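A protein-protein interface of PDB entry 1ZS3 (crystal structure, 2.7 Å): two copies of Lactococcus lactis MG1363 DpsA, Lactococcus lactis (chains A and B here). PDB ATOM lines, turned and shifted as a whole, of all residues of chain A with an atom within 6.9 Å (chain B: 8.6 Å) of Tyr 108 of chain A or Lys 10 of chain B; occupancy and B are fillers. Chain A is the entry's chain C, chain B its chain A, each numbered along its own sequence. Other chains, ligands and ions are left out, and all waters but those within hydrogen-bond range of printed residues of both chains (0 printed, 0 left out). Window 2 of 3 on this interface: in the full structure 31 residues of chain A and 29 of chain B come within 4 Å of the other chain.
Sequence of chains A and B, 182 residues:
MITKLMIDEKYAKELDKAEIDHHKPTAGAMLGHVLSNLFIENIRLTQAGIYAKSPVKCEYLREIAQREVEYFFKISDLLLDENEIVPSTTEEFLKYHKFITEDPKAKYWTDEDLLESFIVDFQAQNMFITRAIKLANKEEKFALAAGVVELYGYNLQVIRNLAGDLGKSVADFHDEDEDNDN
The side-chain hydroxyl (OH) of Tyr 108 of chain A is in hydrogen-bond range of the side-chain carboxylate (OE2) of Glu 14 of chain B, 2.7 Å away.
The backbone carbonyl oxygen (O) of Val 86 of chain B sits at hydrogen-bond distance from the side-chain hydroxyl (OH) of Tyr 51 of chain A (2.6 Å).
NZ of Lys 107 of chain A lies within hydrogen-bond range of O of Val 86 of chain B (3.4 Å).
OG of Ser 88 of chain B lies within hydrogen-bond range of NZ of Lys 107 of chain A, 3.3 Å away.
Hydrophobic or aromatic side chains of chain B that line the printed part of chain A: Ile 7, Tyr 11 and Val 86.
Printed residues of chain A that touch a printed residue of chain B: Tyr 51, Pro 104, Lys 105, Lys 107 and Tyr 108.
Among the printed residues, 12 pairs touch across the chains.
Among the printed residues, no Asp or Glu carboxylate lies within 4 Å of a Lys or Arg side-chain nitrogen of the other chain.
No position is printed for both chains.
Of the 12 pairs that touch across the chains among the printed residues, none has its exchanged pair printed and touching as well.
Among the printed residues, merely in contact across the chains: Lys 107 of chain A with Glu 14 of chain B, Tyr 108 of chain A with Lys 10 of chain B, Tyr 51 of chain A with Ser 88 of chain B, Lys 105 of chain A with Tyr 11 of chain B, Tyr 51 of chain A with Ile 85 of chain B, Pro 104 of chain A with Tyr 11 of chain B, Lys 105 of chain A with Ile 7 of chain B and Tyr 108 of chain A with Tyr 11 of chain B.
Of chain B, only Lys 10, Tyr 11 and Glu 14 come within 4 Å of Tyr 108 of chain A.
Lys 10 of chain B touches one residue of chain A.
Of the printed residues of chain A, Ser 88 of chain B touches Tyr 51 and Lys 107.
Of the printed residues of chain B, Pro 104 of chain A touches Tyr 11.
Of the printed residues of chain B, Lys 105 of chain A touches Ile 7 and Tyr 11.
Printed residues of chain B within 4 Å of Tyr 51 of chain A: Ile 85, Val 86 and Ser 88.
Of the printed residues of chain A, Tyr 11 of chain B touches Pro 104, Lys 105 and Tyr 108.
The nearest residue of chain B that does not touch Tyr 108 of chain A is Ile 7 of chain B (4.1 Å).
The nearest residue of chain A that does not touch Lys 10 of chain B is Lys 53 of chain A (6.7 Å).
The nearest printed residue of chain A that does not touch Ile 7 of chain B is Tyr 108 of chain A (4.1 Å).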
ATOM      1  N   TYR A  51     -15.792  22.801 -21.728  1.00  0.00           N
ATOM      2  CA  TYR A  51     -14.665  23.622 -21.213  1.00  0.00           C
ATOM      3  C   TYR A  51     -13.901  24.411 -22.257  1.00  0.00           C
ATOM      4  O   TYR A  51     -13.301  25.410 -21.902  1.00  0.00           O
ATOM      5  CB  TYR A  51     -13.669  22.787 -20.393  1.00  0.00           C
ATOM      6  CG  TYR A  51     -14.167  22.480 -19.000  1.00  0.00           C
ATOM      7  CD1 TYR A  51     -14.256  23.479 -18.041  1.00  0.00           C
ATOM      8  CD2 TYR A  51     -14.524  21.196 -18.648  1.00  0.00           C
ATOM      9  CE1 TYR A  51     -14.695  23.213 -16.769  1.00  0.00           C
ATOM     10  CE2 TYR A  51     -14.960  20.903 -17.379  1.00  0.00           C
ATOM     11  CZ  TYR A  51     -15.062  21.915 -16.440  1.00  0.00           C
ATOM     12  OH  TYR A  51     -15.529  21.608 -15.175  1.00  0.00           O
ATOM     13  N   LYS A  53     -13.060  27.048 -25.272  1.00  0.00           N
ATOM     14  CA  LYS A  53     -13.412  28.485 -25.179  1.00  0.00           C
ATOM     15  C   LYS A  53     -14.351  28.901 -26.342  1.00  0.00           C
ATOM     16  O   LYS A  53     -15.439  29.428 -26.119  1.00  0.00           O
ATOM     17  CB  LYS A  53     -12.123  29.367 -25.161  1.00  0.00           C
ATOM     18  CG  LYS A  53     -11.414  29.495 -23.765  1.00  0.00           C
ATOM     19  CD  LYS A  53     -11.340  28.196 -22.948  1.00  0.00           C
ATOM     20  CE  LYS A  53     -10.636  28.369 -21.581  1.00  0.00           C
ATOM     21  NZ  LYS A  53      -9.670  27.229 -21.261  1.00  0.00           N
ATOM     22  N   PRO A 104      -8.567  14.941 -15.918  1.00  0.00           N
ATOM     23  CA  PRO A 104      -9.269  16.093 -15.329  1.00  0.00           C
ATOM     24  C   PRO A 104      -8.572  17.447 -15.545  1.00  0.00           C
ATOM     25  O   PRO A 104      -9.190  18.504 -15.414  1.00  0.00           O
ATOM     26  CB  PRO A 104      -9.323  15.755 -13.823  1.00  0.00           C
ATOM     27  CG  PRO A 104      -9.081  14.298 -13.731  1.00  0.00           C
ATOM     28  CD  PRO A 104      -8.181  13.945 -14.902  1.00  0.00           C
ATOM     29  N   LYS A 105      -7.284  17.388 -15.858  1.00  0.00           N
ATOM     30  CA  LYS A 105      -6.508  18.569 -16.146  1.00  0.00           C
ATOM     31  C   LYS A 105      -6.780  19.190 -17.512  1.00  0.00           C
ATOM     32  O   LYS A 105      -6.329  20.305 -17.772  1.00  0.00           O
ATOM     33  CB  LYS A 105      -5.000  18.246 -16.051  1.00  0.00           C
ATOM     34  CG  LYS A 105      -4.375  18.184 -14.640  1.00  0.00           C
ATOM     35  CD  LYS A 105      -2.790  18.134 -14.697  1.00  0.00           C
ATOM     36  CE  LYS A 105      -2.258  16.697 -14.982  1.00  0.00           C
ATOM     37  NZ  LYS A 105      -2.194  15.890 -13.683  1.00  0.00           N
ATOM     38  N   ALA A 106      -7.503  18.487 -18.372  1.00  0.00           N
ATOM     39  CA  ALA A 106      -7.779  18.944 -19.731  1.00  0.00           C
ATOM     40  C   ALA A 106      -8.736  20.125 -19.789  1.00  0.00           C
ATOM     41  O   ALA A 106      -8.776  20.781 -20.823  1.00  0.00           O
ATOM     42  CB  ALA A 106      -8.280  17.831 -20.611  1.00  0.00           C
ATOM     43  N   LYS A 107      -9.472  20.431 -18.701  1.00  0.00           N
ATOM     44  CA  LYS A 107     -10.258  21.689 -18.614  1.00  0.00           C
ATOM     45  C   LYS A 107      -9.465  22.972 -18.862  1.00  0.00           C
ATOM     46  O   LYS A 107     -10.030  23.986 -19.251  1.00  0.00           O
ATOM     47  CB  LYS A 107     -11.076  21.845 -17.324  1.00  0.00           C
ATOM     48  CG  LYS A 107     -10.676  21.012 -16.088  1.00  0.00           C
ATOM     49  CD  LYS A 107     -11.797  21.163 -15.027  1.00  0.00           C
ATOM     50  CE  LYS A 107     -11.719  20.064 -13.998  1.00  0.00           C
ATOM     51  NZ  LYS A 107     -12.773  18.989 -14.165  1.00  0.00           N
ATOM     52  N   TYR A 108      -8.150  22.948 -18.655  1.00  0.00           N
ATOM     53  CA  TYR A 108      -7.290  24.143 -18.801  1.00  0.00           C
ATOM     54  C   TYR A 108      -6.361  24.066 -19.979  1.00  0.00           C
ATOM     55  O   TYR A 108      -5.538  24.961 -20.098  1.00  0.00           O
ATOM     56  CB  TYR A 108      -6.425  24.405 -17.535  1.00  0.00           C
ATOM     57  CG  TYR A 108      -7.187  24.343 -16.249  1.00  0.00           C
ATOM     58  CD1 TYR A 108      -8.082  25.361 -15.907  1.00  0.00           C
ATOM     59  CD2 TYR A 108      -7.034  23.272 -15.384  1.00  0.00           C
ATOM     60  CE1 TYR A 108      -8.792  25.328 -14.717  1.00  0.00           C
ATOM     61  CE2 TYR A 108      -7.737  23.212 -14.204  1.00  0.00           C
ATOM     62  CZ  TYR A 108      -8.618  24.239 -13.857  1.00  0.00           C
ATOM     63  OH  TYR A 108      -9.321  24.162 -12.659  1.00  0.00           O
ATOM     64  N   TRP A 109      -6.485  23.068 -20.852  1.00  0.00           N
ATOM     65  CA  TRP A 109      -5.737  23.056 -22.110  1.00  0.00           C
ATOM     66  C   TRP A 109      -6.288  24.165 -23.009  1.00  0.00           C
ATOM     67  O   TRP A 109      -7.401  24.674 -22.874  1.00  0.00           O
ATOM     68  CB  TRP A 109      -5.773  21.718 -22.871  1.00  0.00           C
ATOM     69  CG  TRP A 109      -5.225  20.498 -22.151  1.00  0.00           C
ATOM     70  CD1 TRP A 109      -4.765  20.448 -20.860  1.00  0.00           C
ATOM     71  CD2 TRP A 109      -5.089  19.153 -22.666  1.00  0.00           C
ATOM     72  NE1 TRP A 109      -4.362  19.172 -20.547  1.00  0.00           N
ATOM     73  CE2 TRP A 109      -4.548  18.360 -21.633  1.00  0.00           C
ATOM     74  CE3 TRP A 109      -5.367  18.538 -23.892  1.00  0.00           C
ATOM     75  CZ2 TRP A 109      -4.286  16.992 -21.781  1.00  0.00           C
ATOM     76  CZ3 TRP A 109      -5.100  17.164 -24.039  1.00  0.00           C
ATOM     77  CH2 TRP A 109      -4.563  16.413 -22.985  1.00  0.00           C
ATOM     78  N   THR A 110      -5.457  24.569 -23.938  1.00  0.00           N
ATOM     79  CA  THR A 110      -5.803  25.534 -24.931  1.00  0.00           C
ATOM     80  C   THR A 110      -6.733  24.815 -25.955  1.00  0.00           C
ATOM     81  O   THR A 110      -6.779  23.589 -25.963  1.00  0.00           O
ATOM     82  CB  THR A 110      -4.487  26.053 -25.510  1.00  0.00           C
ATOM     83  OG1 THR A 110      -4.674  27.327 -26.122  1.00  0.00           O
ATOM     84  CG2 THR A 110      -3.905  25.176 -26.595  1.00  0.00           C
ATOM     85  N   LEU A 114      -6.602  20.627 -27.097  1.00  0.00           N
ATOM     86  CA  LEU A 114      -7.793  19.776 -27.157  1.00  0.00           C
ATOM     87  C   LEU A 114      -8.040  19.176 -28.559  1.00  0.00           C
ATOM     88  O   LEU A 114      -8.280  17.977 -28.691  1.00  0.00           O
ATOM     89  CB  LEU A 114      -8.999  20.542 -26.686  1.00  0.00           C
ATOM     90  CG  LEU A 114      -9.081  20.590 -25.158  1.00  0.00           C
ATOM     91  CD1 LEU A 114     -10.158  21.584 -24.744  1.00  0.00           C
ATOM     92  CD2 LEU A 114      -9.366  19.204 -24.616  1.00  0.00           C
ATOM     93  N   THR B   3       2.150  26.155 -20.236  1.00  0.00           N
ATOM     94  CA  THR B   3       1.852  24.695 -20.169  1.00  0.00           C
ATOM     95  C   THR B   3       2.272  24.125 -18.811  1.00  0.00           C
ATOM     96  O   THR B   3       2.723  24.923 -17.972  1.00  0.00           O
ATOM     97  CB  THR B   3       2.531  23.900 -21.338  1.00  0.00           C
ATOM     98  OG1 THR B   3       3.908  23.617 -21.005  1.00  0.00           O
ATOM     99  CG2 THR B   3       2.621  24.740 -22.666  1.00  0.00           C
ATOM    100  N   LYS B   4       2.133  22.814 -18.632  1.00  0.00           N
ATOM    101  CA  LYS B   4       2.479  21.979 -17.425  1.00  0.00           C
ATOM    102  C   LYS B   4       2.426  22.687 -16.040  1.00  0.00           C
ATOM    103  O   LYS B   4       1.685  22.244 -15.152  1.00  0.00           O
ATOM    104  CB  LYS B   4       3.845  21.276 -17.629  1.00  0.00           C
ATOM    105  CG  LYS B   4       3.919  20.356 -18.861  1.00  0.00           C
ATOM    106  CD  LYS B   4       5.367  19.917 -19.171  1.00  0.00           C
ATOM    107  CE  LYS B   4       5.550  19.620 -20.663  1.00  0.00           C
ATOM    108  NZ  LYS B   4       6.074  18.247 -20.917  1.00  0.00           N
ATOM    109  N   LEU B   5       3.266  23.735 -15.859  1.00  0.00           N
ATOM    110  CA  LEU B   5       3.323  24.576 -14.643  1.00  0.00           C
ATOM    111  C   LEU B   5       2.043  25.396 -14.377  1.00  0.00           C
ATOM    112  O   LEU B   5       1.480  25.299 -13.284  1.00  0.00           O
ATOM    113  CB  LEU B   5       4.542  25.541 -14.700  1.00  0.00           C
ATOM    114  CG  LEU B   5       4.928  26.320 -13.415  1.00  0.00           C
ATOM    115  CD1 LEU B   5       5.476  25.376 -12.307  1.00  0.00           C
ATOM    116  CD2 LEU B   5       5.933  27.436 -13.785  1.00  0.00           C
ATOM    117  N   MET B   6       1.627  26.232 -15.334  1.00  0.00           N
ATOM    118  CA  MET B   6       0.361  26.976 -15.243  1.00  0.00           C
ATOM    119  C   MET B   6      -0.856  26.041 -15.095  1.00  0.00           C
ATOM    120  O   MET B   6      -1.868  26.455 -14.508  1.00  0.00           O
ATOM    121  CB  MET B   6       0.190  27.923 -16.478  1.00  0.00           C
ATOM    122  CG  MET B   6      -0.459  27.239 -17.760  1.00  0.00           C
ATOM    123  SD  MET B   6      -0.102  28.078 -19.386  1.00  0.00           S
ATOM    124  CE  MET B   6      -1.609  27.555 -20.522  1.00  0.00           C
ATOM    125  N   ILE B   7      -0.772  24.827 -15.637  1.00  0.00           N
ATOM    126  CA  ILE B   7      -1.857  23.823 -15.610  1.00  0.00           C
ATOM    127  C   ILE B   7      -1.953  23.059 -14.289  1.00  0.00           C
ATOM    128  O   ILE B   7      -3.043  22.614 -13.879  1.00  0.00           O
ATOM    129  CB  ILE B   7      -1.719  22.845 -16.827  1.00  0.00           C
ATOM    130  CG1 ILE B   7      -2.263  23.477 -18.097  1.00  0.00           C
ATOM    131  CG2 ILE B   7      -2.462  21.529 -16.610  1.00  0.00           C
ATOM    132  CD1 ILE B   7      -1.761  22.855 -19.349  1.00  0.00           C
ATOM    133  N   ASP B   8      -0.803  22.878 -13.618  1.00  0.00           N
ATOM    134  CA  ASP B   8      -0.767  22.183 -12.337  1.00  0.00           C
ATOM    135  C   ASP B   8      -1.137  23.034 -11.147  1.00  0.00           C
ATOM    136  O   ASP B   8      -1.676  22.507 -10.179  1.00  0.00           O
ATOM    137  CB  ASP B   8       0.587  21.576 -12.120  1.00  0.00           C
ATOM    138  CG  ASP B   8       0.654  20.162 -12.595  1.00  0.00           C
ATOM    139  OD1 ASP B   8       0.049  19.305 -11.938  1.00  0.00           O
ATOM    140  OD2 ASP B   8       1.317  19.826 -13.597  1.00  0.00           O
ATOM    141  N   GLU B   9      -0.859  24.334 -11.243  1.00  0.00           N
ATOM    142  CA  GLU B   9      -1.277  25.300 -10.228  1.00  0.00           C
ATOM    143  C   GLU B   9      -2.776  25.546 -10.318  1.00  0.00           C
ATOM    144  O   GLU B   9      -3.433  25.548  -9.278  1.00  0.00           O
ATOM    145  CB  GLU B   9      -0.442  26.611 -10.270  1.00  0.00           C
ATOM    146  CG  GLU B   9      -0.574  27.471 -11.544  1.00  0.00           C
ATOM    147  CD  GLU B   9      -0.060  28.906 -11.373  1.00  0.00           C
ATOM    148  OE1 GLU B   9      -0.887  29.777 -11.001  1.00  0.00           O
ATOM    149  OE2 GLU B   9       1.147  29.168 -11.612  1.00  0.00           O
ATOM    150  N   LYS B  10      -3.311  25.687 -11.542  1.00  0.00           N
ATOM    151  CA  LYS B  10      -4.759  25.859 -11.718  1.00  0.00           C
ATOM    152  C   LYS B  10      -5.512  24.635 -11.178  1.00  0.00           C
ATOM    153  O   LYS B  10      -6.539  24.779 -10.518  1.00  0.00           O
ATOM    154  CB  LYS B  10      -5.093  26.133 -13.197  1.00  0.00           C
ATOM    155  CG  LYS B  10      -4.844  27.588 -13.656  1.00  0.00           C
ATOM    156  CD  LYS B  10      -5.112  27.789 -15.191  1.00  0.00           C
ATOM    157  CE  LYS B  10      -6.270  28.801 -15.496  1.00  0.00           C
ATOM    158  NZ  LYS B  10      -5.867  29.916 -16.421  1.00  0.00           N
ATOM    159  N   TYR B  11      -4.959  23.432 -11.422  1.00  0.00           N
ATOM    160  CA  TYR B  11      -5.595  22.162 -10.963  1.00  0.00           C
ATOM    161  C   TYR B  11      -5.520  21.931  -9.427  1.00  0.00           C
ATOM    162  O   TYR B  11      -6.494  21.494  -8.795  1.00  0.00           O
ATOM    163  CB  TYR B  11      -4.981  20.960 -11.703  1.00  0.00           C
ATOM    164  CG  TYR B  11      -5.665  19.646 -11.362  1.00  0.00           C
ATOM    165  CD1 TYR B  11      -4.958  18.553 -10.860  1.00  0.00           C
ATOM    166  CD2 TYR B  11      -7.046  19.519 -11.488  1.00  0.00           C
ATOM    167  CE1 TYR B  11      -5.617  17.362 -10.516  1.00  0.00           C
ATOM    168  CE2 TYR B  11      -7.699  18.346 -11.150  1.00  0.00           C
ATOM    169  CZ  TYR B  11      -6.985  17.281 -10.667  1.00  0.00           C
ATOM    170  OH  TYR B  11      -7.664  16.143 -10.353  1.00  0.00           O
ATOM    171  N   ALA B  12      -4.379  22.243  -8.819  1.00  0.00           N
ATOM    172  CA  ALA B  12      -4.191  22.008  -7.401  1.00  0.00           C
ATOM    173  C   ALA B  12      -4.993  23.055  -6.624  1.00  0.00           C
ATOM    174  O   ALA B  12      -5.379  22.824  -5.473  1.00  0.00           O
ATOM    175  CB  ALA B  12      -2.729  22.020  -7.042  1.00  0.00           C
ATOM    176  N   LYS B  13      -5.247  24.198  -7.256  1.00  0.00           N
ATOM    177  CA  LYS B  13      -6.024  25.273  -6.660  1.00  0.00           C
ATOM    178  C   LYS B  13      -7.520  25.016  -6.786  1.00  0.00           C
ATOM    179  O   LYS B  13      -8.320  25.589  -6.036  1.00  0.00           O
ATOM    180  CB  LYS B  13      -5.657  26.652  -7.252  1.00  0.00           C
ATOM    181  CG  LYS B  13      -5.578  27.800  -6.242  1.00  0.00           C
ATOM    182  CD  LYS B  13      -5.545  29.164  -6.919  1.00  0.00           C
ATOM    183  CE  LYS B  13      -6.948  29.735  -7.018  1.00  0.00           C
ATOM    184  NZ  LYS B  13      -6.944  31.199  -7.307  1.00  0.00           N
ATOM    185  N   GLU B  14      -7.881  24.174  -7.763  1.00  0.00           N
ATOM    186  CA  GLU B  14      -9.256  23.752  -8.006  1.00  0.00           C
ATOM    187  C   GLU B  14      -9.622  22.690  -6.996  1.00  0.00           C
ATOM    188  O   GLU B  14     -10.659  22.806  -6.358  1.00  0.00           O
ATOM    189  CB  GLU B  14      -9.388  23.198  -9.425  1.00  0.00           C
ATOM    190  CG  GLU B  14     -10.729  22.540  -9.764  1.00  0.00           C
ATOM    191  CD  GLU B  14     -10.622  21.409 -10.781  1.00  0.00           C
ATOM    192  OE1 GLU B  14     -11.087  20.296 -10.459  1.00  0.00           O
ATOM    193  OE2 GLU B  14     -10.093  21.639 -11.892  1.00  0.00           O
ATOM    194  N   LEU B  15      -8.753  21.675  -6.882  1.00  0.00           N
ATOM    195  CA  LEU B  15      -8.879  20.585  -5.877  1.00  0.00           C
ATOM    196  C   LEU B  15      -8.892  21.053  -4.419  1.00  0.00           C
ATOM    197  O   LEU B  15      -9.534  20.420  -3.572  1.00  0.00           O
ATOM    198  CB  LEU B  15      -7.713  19.621  -6.016  1.00  0.00           C
ATOM    199  CG  LEU B  15      -7.922  18.528  -7.059  1.00  0.00           C
ATOM    200  CD1 LEU B  15      -6.558  17.918  -7.421  1.00  0.00           C
ATOM    201  CD2 LEU B  15      -8.940  17.462  -6.594  1.00  0.00           C
ATOM    202  N   ASP B  16      -8.186  22.144  -4.160  1.00  0.00           N
ATOM    203  CA  ASP B  16      -8.131  22.753  -2.851  1.00  0.00           C
ATOM    204  C   ASP B  16      -9.503  23.377  -2.611  1.00  0.00           C
ATOM    205  O   ASP B  16     -10.188  23.009  -1.668  1.00  0.00           O
ATOM    206  CB  ASP B  16      -7.003  23.806  -2.819  1.00  0.00           C
ATOM    207  CG  ASP B  16      -6.316  23.885  -1.468  1.00  0.00           C
ATOM    208  OD1 ASP B  16      -6.483  24.925  -0.765  1.00  0.00           O
ATOM    209  OD2 ASP B  16      -5.573  22.958  -1.031  1.00  0.00           O
ATOM    210  N   LYS B  17      -9.884  24.279  -3.515  1.00  0.00           N
ATOM    211  CA  LYS B  17     -11.142  24.984  -3.472  1.00  0.00           C
ATOM    212  C   LYS B  17     -12.339  24.039  -3.475  1.00  0.00           C
ATOM    213  O   LYS B  17     -13.381  24.351  -2.891  1.00  0.00           O
ATOM    214  CB  LYS B  17     -11.252  25.985  -4.649  1.00  0.00           C
ATOM    215  CG  LYS B  17     -12.098  27.245  -4.364  1.00  0.00           C
ATOM    216  CD  LYS B  17     -12.349  28.039  -5.641  1.00  0.00           C
ATOM    217  CE  LYS B  17     -13.741  27.780  -6.155  1.00  0.00           C
ATOM    218  NZ  LYS B  17     -14.734  28.468  -5.281  1.00  0.00           N
ATOM    219  N   GLU B  84     -18.645  28.280 -12.093  1.00  0.00           N
ATOM    220  CA  GLU B  84     -18.340  27.148 -11.269  1.00  0.00           C
ATOM    221  C   GLU B  84     -17.677  26.166 -12.196  1.00  0.00           C
ATOM    222  O   GLU B  84     -17.428  26.439 -13.394  1.00  0.00           O
ATOM    223  CB  GLU B  84     -19.585  26.525 -10.602  1.00  0.00           C
ATOM    224  CG  GLU B  84     -20.254  27.370  -9.498  1.00  0.00           C
ATOM    225  CD  GLU B  84     -19.341  27.644  -8.311  1.00  0.00           C
ATOM    226  OE1 GLU B  84     -18.758  26.687  -7.743  1.00  0.00           O
ATOM    227  OE2 GLU B  84     -19.193  28.835  -7.954  1.00  0.00           O
ATOM    228  N   ILE B  85     -17.381  25.026 -11.595  1.00  0.00           N
ATOM    229  CA  ILE B  85     -16.612  23.968 -12.163  1.00  0.00           C
ATOM    230  C   ILE B  85     -17.415  22.703 -12.035  1.00  0.00           C
ATOM    231  O   ILE B  85     -18.320  22.571 -11.193  1.00  0.00           O
ATOM    232  CB  ILE B  85     -15.243  23.872 -11.410  1.00  0.00           C
ATOM    233  CG1 ILE B  85     -14.101  24.336 -12.332  1.00  0.00           C
ATOM    234  CG2 ILE B  85     -14.977  22.475 -10.824  1.00  0.00           C
ATOM    235  CD1 ILE B  85     -13.985  25.856 -12.512  1.00  0.00           C
ATOM    236  N   VAL B  86     -17.101  21.791 -12.926  1.00  0.00           N
ATOM    237  CA  VAL B  86     -17.998  20.704 -13.238  1.00  0.00           C
ATOM    238  C   VAL B  86     -17.213  19.406 -13.382  1.00  0.00           C
ATOM    239  O   VAL B  86     -16.134  19.390 -13.993  1.00  0.00           O
ATOM    240  CB  VAL B  86     -18.805  21.102 -14.507  1.00  0.00           C
ATOM    241  CG1 VAL B  86     -19.017  19.949 -15.460  1.00  0.00           C
ATOM    242  CG2 VAL B  86     -20.138  21.714 -14.090  1.00  0.00           C
ATOM    243  N   SER B  88     -16.008  16.167 -15.048  1.00  0.00           N
ATOM    244  CA  SER B  88     -15.939  15.929 -16.482  1.00  0.00           C
ATOM    245  C   SER B  88     -15.078  14.737 -16.881  1.00  0.00           C
ATOM    246  O   SER B  88     -14.607  14.685 -18.041  1.00  0.00           O
ATOM    247  CB  SER B  88     -15.361  17.175 -17.132  1.00  0.00           C
ATOM    248  OG  SER B  88     -14.018  17.379 -16.750  1.00  0.00           O
